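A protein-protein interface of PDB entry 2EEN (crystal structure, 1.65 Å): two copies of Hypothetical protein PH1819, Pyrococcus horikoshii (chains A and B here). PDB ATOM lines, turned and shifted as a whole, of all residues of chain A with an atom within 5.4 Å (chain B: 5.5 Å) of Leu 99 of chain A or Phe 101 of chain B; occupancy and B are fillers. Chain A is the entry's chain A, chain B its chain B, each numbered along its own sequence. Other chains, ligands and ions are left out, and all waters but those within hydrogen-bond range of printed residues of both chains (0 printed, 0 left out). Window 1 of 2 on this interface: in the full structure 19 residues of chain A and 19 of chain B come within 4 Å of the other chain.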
ATOM      1  N   PRO A  38     -13.242 -20.681  24.106  1.00  0.00           N
ATOM      2  CA  PRO A  38     -11.843 -20.892  23.725  1.00  0.00           C
ATOM      3  C   PRO A  38     -10.966 -19.644  23.748  1.00  0.00           C
ATOM      4  O   PRO A  38      -9.752 -19.741  23.928  1.00  0.00           O
ATOM      5  CB  PRO A  38     -11.959 -21.476  22.318  1.00  0.00           C
ATOM      6  CG  PRO A  38     -13.206 -20.811  21.785  1.00  0.00           C
ATOM      7  CD  PRO A  38     -14.147 -20.936  22.973  1.00  0.00           C
ATOM      8  N   GLU A  94     -19.434 -32.981  20.172  1.00  0.00           N
ATOM      9  CA  GLU A  94     -18.223 -33.038  19.367  1.00  0.00           C
ATOM     10  C   GLU A  94     -17.918 -31.681  18.727  1.00  0.00           C
ATOM     11  O   GLU A  94     -16.766 -31.251  18.682  1.00  0.00           O
ATOM     12  CB  GLU A  94     -18.374 -34.118  18.291  1.00  0.00           C
ATOM     13  CG  GLU A  94     -17.120 -34.388  17.485  1.00  0.00           C
ATOM     14  CD  GLU A  94     -17.299 -35.535  16.506  1.00  0.00           C
ATOM     15  OE1 GLU A  94     -18.305 -35.536  15.763  1.00  0.00           O
ATOM     16  OE2 GLU A  94     -16.434 -36.433  16.475  1.00  0.00           O
ATOM     17  N   LEU A  95     -18.955 -31.010  18.242  1.00  0.00           N
ATOM     18  CA  LEU A  95     -18.788 -29.707  17.609  1.00  0.00           C
ATOM     19  C   LEU A  95     -18.186 -28.703  18.587  1.00  0.00           C
ATOM     20  O   LEU A  95     -17.222 -28.003  18.273  1.00  0.00           O
ATOM     21  CB  LEU A  95     -20.137 -29.189  17.104  1.00  0.00           C
ATOM     22  CG  LEU A  95     -20.109 -27.786  16.494  1.00  0.00           C
ATOM     23  CD1 LEU A  95     -19.063 -27.732  15.387  1.00  0.00           C
ATOM     24  CD2 LEU A  95     -21.489 -27.436  15.955  1.00  0.00           C
ATOM     25  N   LEU A  96     -18.762 -28.627  19.777  1.00  0.00           N
ATOM     26  CA  LEU A  96     -18.249 -27.712  20.781  1.00  0.00           C
ATOM     27  C   LEU A  96     -16.785 -28.020  21.095  1.00  0.00           C
ATOM     28  O   LEU A  96     -15.966 -27.119  21.175  1.00  0.00           O
ATOM     29  CB  LEU A  96     -19.096 -27.792  22.055  1.00  0.00           C
ATOM     30  CG  LEU A  96     -20.500 -27.188  21.948  1.00  0.00           C
ATOM     31  CD1 LEU A  96     -21.198 -27.274  23.295  1.00  0.00           C
ATOM     32  CD2 LEU A  96     -20.397 -25.734  21.507  1.00  0.00           C
ATOM     33  N   ASP A  97     -16.456 -29.299  21.245  1.00  0.00           N
ATOM     34  CA  ASP A  97     -15.084 -29.688  21.551  1.00  0.00           C
ATOM     35  C   ASP A  97     -14.123 -29.240  20.448  1.00  0.00           C
ATOM     36  O   ASP A  97     -13.077 -28.653  20.720  1.00  0.00           O
ATOM     37  CB  ASP A  97     -14.997 -31.206  21.735  1.00  0.00           C
ATOM     38  CG  ASP A  97     -13.676 -31.643  22.337  1.00  0.00           C
ATOM     39  OD1 ASP A  97     -13.347 -31.174  23.448  1.00  0.00           O
ATOM     40  OD2 ASP A  97     -12.970 -32.454  21.701  1.00  0.00           O
ATOM     41  N   ARG A  98     -14.492 -29.511  19.200  1.00  0.00           N
ATOM     42  CA  ARG A  98     -13.666 -29.142  18.057  1.00  0.00           C
ATOM     43  C   ARG A  98     -13.477 -27.636  17.957  1.00  0.00           C
ATOM     44  O   ARG A  98     -12.415 -27.164  17.552  1.00  0.00           O
ATOM     45  CB  ARG A  98     -14.289 -29.668  16.762  1.00  0.00           C
ATOM     46  CG  ARG A  98     -14.255 -31.183  16.624  1.00  0.00           C
ATOM     47  CD  ARG A  98     -12.832 -31.693  16.470  1.00  0.00           C
ATOM     48  NE  ARG A  98     -12.789 -33.144  16.293  1.00  0.00           N
ATOM     49  CZ  ARG A  98     -11.683 -33.837  16.039  1.00  0.00           C
ATOM     50  NH1 ARG A  98     -10.516 -33.215  15.931  1.00  0.00           N
ATOM     51  NH2 ARG A  98     -11.742 -35.154  15.895  1.00  0.00           N
ATOM     52  N   LEU A  99     -14.503 -26.878  18.326  1.00  0.00           N
ATOM     53  CA  LEU A  99     -14.415 -25.425  18.275  1.00  0.00           C
ATOM     54  C   LEU A  99     -13.626 -24.847  19.446  1.00  0.00           C
ATOM     55  O   LEU A  99     -13.385 -23.649  19.511  1.00  0.00           O
ATOM     56  CB  LEU A  99     -15.815 -24.814  18.213  1.00  0.00           C
ATOM     57  CG  LEU A  99     -16.553 -25.109  16.907  1.00  0.00           C
ATOM     58  CD1 LEU A  99     -17.959 -24.537  16.965  1.00  0.00           C
ATOM     59  CD2 LEU A  99     -15.794 -24.510  15.736  1.00  0.00           C
ATOM     60  N   GLY A 100     -13.222 -25.703  20.378  1.00  0.00           N
ATOM     61  CA  GLY A 100     -12.426 -25.222  21.492  1.00  0.00           C
ATOM     62  C   GLY A 100     -13.160 -24.940  22.785  1.00  0.00           C
ATOM     63  O   GLY A 100     -12.571 -24.392  23.722  1.00  0.00           O
ATOM     64  N   PHE A 101     -14.444 -25.280  22.833  1.00  0.00           N
ATOM     65  CA  PHE A 101     -15.224 -25.082  24.044  1.00  0.00           C
ATOM     66  C   PHE A 101     -14.992 -26.309  24.890  1.00  0.00           C
ATOM     67  O   PHE A 101     -15.324 -27.426  24.493  1.00  0.00           O
ATOM     68  CB  PHE A 101     -16.710 -24.939  23.725  1.00  0.00           C
ATOM     69  CG  PHE A 101     -17.040 -23.675  23.015  1.00  0.00           C
ATOM     70  CD1 PHE A 101     -16.827 -23.557  21.644  1.00  0.00           C
ATOM     71  CD2 PHE A 101     -17.495 -22.570  23.723  1.00  0.00           C
ATOM     72  CE1 PHE A 101     -17.068 -22.350  20.989  1.00  0.00           C
ATOM     73  CE2 PHE A 101     -17.735 -21.363  23.079  1.00  0.00           C
ATOM     74  CZ  PHE A 101     -17.518 -21.251  21.710  1.00  0.00           C
ATOM     75  N   TYR B  35     -18.075 -18.856   8.596  1.00  0.00           N
ATOM     76  CA  TYR B  35     -17.679 -18.093   9.758  1.00  0.00           C
ATOM     77  C   TYR B  35     -16.208 -18.185  10.089  1.00  0.00           C
ATOM     78  O   TYR B  35     -15.528 -19.150   9.740  1.00  0.00           O
ATOM     79  CB  TYR B  35     -18.482 -18.577  10.967  1.00  0.00           C
ATOM     80  CG  TYR B  35     -19.957 -18.326  10.822  1.00  0.00           C
ATOM     81  CD1 TYR B  35     -20.516 -17.108  11.210  1.00  0.00           C
ATOM     82  CD2 TYR B  35     -20.789 -19.282  10.248  1.00  0.00           C
ATOM     83  CE1 TYR B  35     -21.867 -16.847  11.023  1.00  0.00           C
ATOM     84  CE2 TYR B  35     -22.139 -19.033  10.058  1.00  0.00           C
ATOM     85  CZ  TYR B  35     -22.671 -17.818  10.445  1.00  0.00           C
ATOM     86  OH  TYR B  35     -24.003 -17.569  10.236  1.00  0.00           O
ATOM     87  N   GLN B  36     -15.722 -17.137  10.741  1.00  0.00           N
ATOM     88  CA  GLN B  36     -14.355 -17.105  11.219  1.00  0.00           C
ATOM     89  C   GLN B  36     -14.493 -17.403  12.707  1.00  0.00           C
ATOM     90  O   GLN B  36     -15.473 -17.010  13.350  1.00  0.00           O
ATOM     91  CB  GLN B  36     -13.724 -15.726  11.035  1.00  0.00           C
ATOM     92  CG  GLN B  36     -12.360 -15.577  11.707  1.00  0.00           C
ATOM     93  CD  GLN B  36     -11.313 -16.539  11.152  1.00  0.00           C
ATOM     94  OE1 GLN B  36     -11.408 -17.753  11.331  1.00  0.00           O
ATOM     95  NE2 GLN B  36     -10.314 -15.995  10.470  1.00  0.00           N
ATOM     96  N   HIS B  37     -13.511 -18.111  13.238  1.00  0.00           N
ATOM     97  CA  HIS B  37     -13.480 -18.484  14.640  1.00  0.00           C
ATOM     98  C   HIS B  37     -13.114 -17.252  15.462  1.00  0.00           C
ATOM     99  O   HIS B  37     -12.380 -16.383  15.001  1.00  0.00           O
ATOM    100  CB  HIS B  37     -12.448 -19.594  14.812  1.00  0.00           C
ATOM    101  CG  HIS B  37     -12.473 -20.260  16.149  1.00  0.00           C
ATOM    102  ND1 HIS B  37     -11.826 -19.740  17.248  1.00  0.00           N
ATOM    103  CD2 HIS B  37     -13.029 -21.426  16.551  1.00  0.00           C
ATOM    104  CE1 HIS B  37     -11.980 -20.563  18.273  1.00  0.00           C
ATOM    105  NE2 HIS B  37     -12.705 -21.592  17.876  1.00  0.00           N
ATOM    106  N   PRO B  38     -13.639 -17.155  16.690  1.00  0.00           N
ATOM    107  CA  PRO B  38     -13.330 -15.996  17.533  1.00  0.00           C
ATOM    108  C   PRO B  38     -11.850 -15.707  17.780  1.00  0.00           C
ATOM    109  O   PRO B  38     -11.485 -14.558  18.026  1.00  0.00           O
ATOM    110  CB  PRO B  38     -14.119 -16.270  18.819  1.00  0.00           C
ATOM    111  CG  PRO B  38     -14.375 -17.742  18.792  1.00  0.00           C
ATOM    112  CD  PRO B  38     -14.619 -18.037  17.339  1.00  0.00           C
ATOM    113  N   ARG B  40      -9.098 -18.422  16.584  1.00  0.00           N
ATOM    114  CA  ARG B  40      -8.271 -19.251  15.717  1.00  0.00           C
ATOM    115  C   ARG B  40      -8.537 -18.709  14.330  1.00  0.00           C
ATOM    116  O   ARG B  40      -9.679 -18.410  14.000  1.00  0.00           O
ATOM    117  CB  ARG B  40      -8.714 -20.719  15.733  1.00  0.00           C
ATOM    118  CG  ARG B  40      -8.194 -21.551  16.879  1.00  0.00           C
ATOM    119  CD  ARG B  40      -7.960 -22.989  16.422  1.00  0.00           C
ATOM    120  NE  ARG B  40      -9.179 -23.677  15.994  1.00  0.00           N
ATOM    121  CZ  ARG B  40     -10.163 -24.033  16.814  1.00  0.00           C
ATOM    122  NH1 ARG B  40     -10.078 -23.762  18.111  1.00  0.00           N
ATOM    123  NH2 ARG B  40     -11.221 -24.679  16.344  1.00  0.00           N
ATOM    124  N   PHE B  42      -9.220 -19.648  11.067  1.00  0.00           N
ATOM    125  CA  PHE B  42      -9.560 -20.842  10.310  1.00  0.00           C
ATOM    126  C   PHE B  42      -8.808 -20.923   8.991  1.00  0.00           C
ATOM    127  O   PHE B  42      -8.565 -22.018   8.485  1.00  0.00           O
ATOM    128  CB  PHE B  42     -11.066 -20.898  10.025  1.00  0.00           C
ATOM    129  CG  PHE B  42     -11.893 -21.469  11.148  1.00  0.00           C
ATOM    130  CD1 PHE B  42     -11.298 -22.105  12.234  1.00  0.00           C
ATOM    131  CD2 PHE B  42     -13.284 -21.409  11.091  1.00  0.00           C
ATOM    132  CE1 PHE B  42     -12.072 -22.680  13.238  1.00  0.00           C
ATOM    133  CE2 PHE B  42     -14.069 -21.983  12.092  1.00  0.00           C
ATOM    134  CZ  PHE B  42     -13.461 -22.618  13.167  1.00  0.00           C
ATOM    135  N   LEU B  49     -16.423 -23.509   9.331  1.00  0.00           N
ATOM    136  CA  LEU B  49     -17.683 -23.637  10.046  1.00  0.00           C
ATOM    137  C   LEU B  49     -18.678 -22.884   9.199  1.00  0.00           C
ATOM    138  O   LEU B  49     -18.483 -21.711   8.899  1.00  0.00           O
ATOM    139  CB  LEU B  49     -17.615 -23.007  11.437  1.00  0.00           C
ATOM    140  CG  LEU B  49     -18.912 -23.157  12.241  1.00  0.00           C
ATOM    141  CD1 LEU B  49     -19.190 -24.627  12.591  1.00  0.00           C
ATOM    142  CD2 LEU B  49     -18.779 -22.340  13.506  1.00  0.00           C
ATOM    143  N   TYR B  66     -19.126 -28.357  10.605  1.00  0.00           N
ATOM    144  CA  TYR B  66     -17.749 -28.058  10.958  1.00  0.00           C
ATOM    145  C   TYR B  66     -16.856 -28.944  10.105  1.00  0.00           C
ATOM    146  O   TYR B  66     -17.130 -30.133   9.942  1.00  0.00           O
ATOM    147  CB  TYR B  66     -17.472 -28.376  12.423  1.00  0.00           C
ATOM    148  CG  TYR B  66     -16.000 -28.397  12.743  1.00  0.00           C
ATOM    149  CD1 TYR B  66     -15.286 -27.214  12.922  1.00  0.00           C
ATOM    150  CD2 TYR B  66     -15.306 -29.605  12.818  1.00  0.00           C
ATOM    151  CE1 TYR B  66     -13.916 -27.232  13.166  1.00  0.00           C
ATOM    152  CE2 TYR B  66     -13.938 -29.635  13.058  1.00  0.00           C
ATOM    153  CZ  TYR B  66     -13.250 -28.448  13.230  1.00  0.00           C
ATOM    154  OH  TYR B  66     -11.892 -28.482  13.455  1.00  0.00           O
ATOM    155  N   LEU B  96     -24.049 -17.879  17.241  1.00  0.00           N
ATOM    156  CA  LEU B  96     -22.721 -17.753  16.657  1.00  0.00           C
ATOM    157  C   LEU B  96     -22.153 -16.349  16.857  1.00  0.00           C
ATOM    158  O   LEU B  96     -20.976 -16.191  17.200  1.00  0.00           O
ATOM    159  CB  LEU B  96     -22.762 -18.091  15.166  1.00  0.00           C
ATOM    160  CG  LEU B  96     -22.957 -19.580  14.871  1.00  0.00           C
ATOM    161  CD1 LEU B  96     -23.126 -19.791  13.382  1.00  0.00           C
ATOM    162  CD2 LEU B  96     -21.757 -20.366  15.380  1.00  0.00           C
ATOM    163  N   ASP B  97     -22.988 -15.332  16.656  1.00  0.00           N
ATOM    164  CA  ASP B  97     -22.533 -13.960  16.823  1.00  0.00           C
ATOM    165  C   ASP B  97     -22.131 -13.704  18.270  1.00  0.00           C
ATOM    166  O   ASP B  97     -21.087 -13.101  18.528  1.00  0.00           O
ATOM    167  CB  ASP B  97     -23.618 -12.966  16.417  1.00  0.00           C
ATOM    168  CG  ASP B  97     -23.078 -11.556  16.289  1.00  0.00           C
ATOM    169  OD1 ASP B  97     -22.235 -11.317  15.395  1.00  0.00           O
ATOM    170  OD2 ASP B  97     -23.480 -10.688  17.089  1.00  0.00           O
ATOM    171  N   LEU B  99     -21.069 -15.807  20.392  1.00  0.00           N
ATOM    172  CA  LEU B  99     -19.858 -16.547  20.731  1.00  0.00           C
ATOM    173  C   LEU B  99     -18.617 -16.020  20.025  1.00  0.00           C
ATOM    174  O   LEU B  99     -17.525 -16.561  20.195  1.00  0.00           O
ATOM    175  CB  LEU B  99     -20.051 -18.037  20.436  1.00  0.00           C
ATOM    176  CG  LEU B  99     -21.083 -18.699  21.355  1.00  0.00           C
ATOM    177  CD1 LEU B  99     -21.291 -20.156  20.960  1.00  0.00           C
ATOM    178  CD2 LEU B  99     -20.615 -18.601  22.797  1.00  0.00           C
ATOM    179  N   GLY B 100     -18.790 -14.969  19.226  1.00  0.00           N
ATOM    180  CA  GLY B 100     -17.656 -14.371  18.547  1.00  0.00           C
ATOM    181  C   GLY B 100     -17.342 -14.847  17.149  1.00  0.00           C
ATOM    182  O   GLY B 100     -16.310 -14.472  16.594  1.00  0.00           O
ATOM    183  N   PHE B 101     -18.205 -15.679  16.577  1.00  0.00           N
ATOM    184  CA  PHE B 101     -17.974 -16.142  15.219  1.00  0.00           C
ATOM    185  C   PHE B 101     -18.503 -15.056  14.309  1.00  0.00           C
ATOM    186  O   PHE B 101     -19.604 -14.542  14.508  1.00  0.00           O
ATOM    187  CB  PHE B 101     -18.699 -17.458  14.939  1.00  0.00           C
ATOM    188  CG  PHE B 101     -18.135 -18.626  15.689  1.00  0.00           C
ATOM    189  CD1 PHE B 101     -18.452 -18.830  17.030  1.00  0.00           C
ATOM    190  CD2 PHE B 101     -17.249 -19.496  15.067  1.00  0.00           C
ATOM    191  CE1 PHE B 101     -17.892 -19.888  17.743  1.00  0.00           C
ATOM    192  CE2 PHE B 101     -16.681 -20.560  15.769  1.00  0.00           C
ATOM    193  CZ  PHE B 101     -17.003 -20.756  17.111  1.00  0.00           C
ATOM    194  N   LYS B 102     -17.714 -14.699  13.311  1.00  0.00           N
ATOM    195  CA  LYS B 102     -18.138 -13.656  12.404  1.00  0.00           C
ATOM    196  C   LYS B 102     -18.208 -14.149  10.981  1.00  0.00           C
ATOM    197  O   LYS B 102     -17.395 -14.970  10.553  1.00  0.00           O
ATOM    198  CB  LYS B 102     -17.197 -12.459  12.514  1.00  0.00           C
ATOM    199  CG  LYS B 102     -17.352 -11.730  13.845  1.00  0.00           C
ATOM    200  CD  LYS B 102     -18.790 -11.245  14.020  1.00  0.00           C
ATOM    201  CE  LYS B 102     -19.072 -10.785  15.447  1.00  0.00           C
ATOM    202  NZ  LYS B 102     -19.048 -11.919  16.414  1.00  0.00           N
ATOM    203  N   GLU B 103     -19.199 -13.648  10.256  1.00  0.00           N
ATOM    204  CA  GLU B 103     -19.379 -14.021   8.869  1.00  0.00           C
ATOM    205  C   GLU B 103     -18.192 -13.555   8.057  1.00  0.00           C
ATOM    206  O   GLU B 103     -17.794 -12.390   8.128  1.00  0.00           O
ATOM    207  CB  GLU B 103     -20.645 -13.391   8.302  1.00  0.00           C
ATOM    208  CG  GLU B 103     -21.919 -14.063   8.732  1.00  0.00           C
ATOM    209  CD  GLU B 103     -23.133 -13.449   8.067  1.00  0.00           C
ATOM    210  OE1 GLU B 103     -23.038 -13.097   6.870  1.00  0.00           O
ATOM    211  OE2 GLU B 103     -24.176 -13.330   8.739  1.00  0.00           O
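The guanidinium group (NH2) of Arg 40 of chain B is in hydrogen-bond range of the backbone carbonyl oxygen (O) of Arg 98 of chain A, 3.0 Å away. O of Leu 99 of chain A sits at hydrogen-bond distance from NE2 of His 37 of chain B.
OE1 of Gln 36 of chain B sits close to O of Arg 40 of chain B (3.2 Å). The side-chain amide oxygen (OE1) of Gln 36 of chain B lies within hydrogen-bond range of the backbone NH (N) of Phe 42 of chain B. The backbone NH (N) of Arg 40 of chain B lies within hydrogen-bond range of a ring nitrogen (ND1) of His 37 of chain B (3.1 Å). The backbone carbonyl oxygen of Leu 96 of chain B lies within hydrogen-bond range of the backbone NH of Phe 101 of chain B (2.9 Å).
Among the printed residues, merely in contact across the chains: Pro 38 of chain A with His 37 of chain B, Leu 95 of chain A with Tyr 66 of chain B, Arg 98 of chain A with Tyr 66 of chain B, Leu 99 of chain A with Arg 40 of chain B, Leu 99 of chain A with Phe 42 of chain B, Leu 99 of chain A with Tyr 66 of chain B, Leu 99 of chain A with Phe 101 of chain B and Phe 101 of chain A with Leu 99 of chain B.
Leu 99 of chain A touches five residues of chain B. Phe 101 of chain B touches just one residue of chain A: Leu 99 (3.9 Å). Of the printed residues of chain A, Phe 42 of chain B touches Leu 99. Printed residues of chain A within 4 Å of Arg 40 of chain B: Arg 98 (3.0 Å) and Leu 99 (3.6 Å). Of the printed residues of chain A, Tyr 66 of chain B touches Leu 95 (3.4 Å), Arg 98 (3.7 Å) and Leu 99 (3.9 Å). Of the printed residues of chain A, His 37 of chain B touches Pro 38 (3.7 Å) and Leu 99 (2.7 Å). The nearest residue of chain A that does not touch Phe 101 of chain B is Phe 101 of chain A (4.2 Å). The nearest printed residue of chain A that does not touch Leu 99 of chain B is Leu 96 of chain A (5.7 Å).
Printed residues of chain B that touch a printed residue of chain A: His 37, Arg 40, Phe 42, Tyr 66, Leu 99 and Phe 101. Hydrophobic or aromatic side chains of chain A that line the printed part of chain B: Pro 38, Leu 95, Leu 99 and Phe 101. Along chain A the printed residues that touch a printed residue of chain B span positions 38 to 101. Among the printed residues, 10 pairs touch across the chains.
Leu 99 of chain A touches Phe 101 of chain B, and with the chains exchanged Phe 101 of chain A touches Leu 99 of chain B. Positions printed for both chains: 38, 96, 97, 99, 100 and 101.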
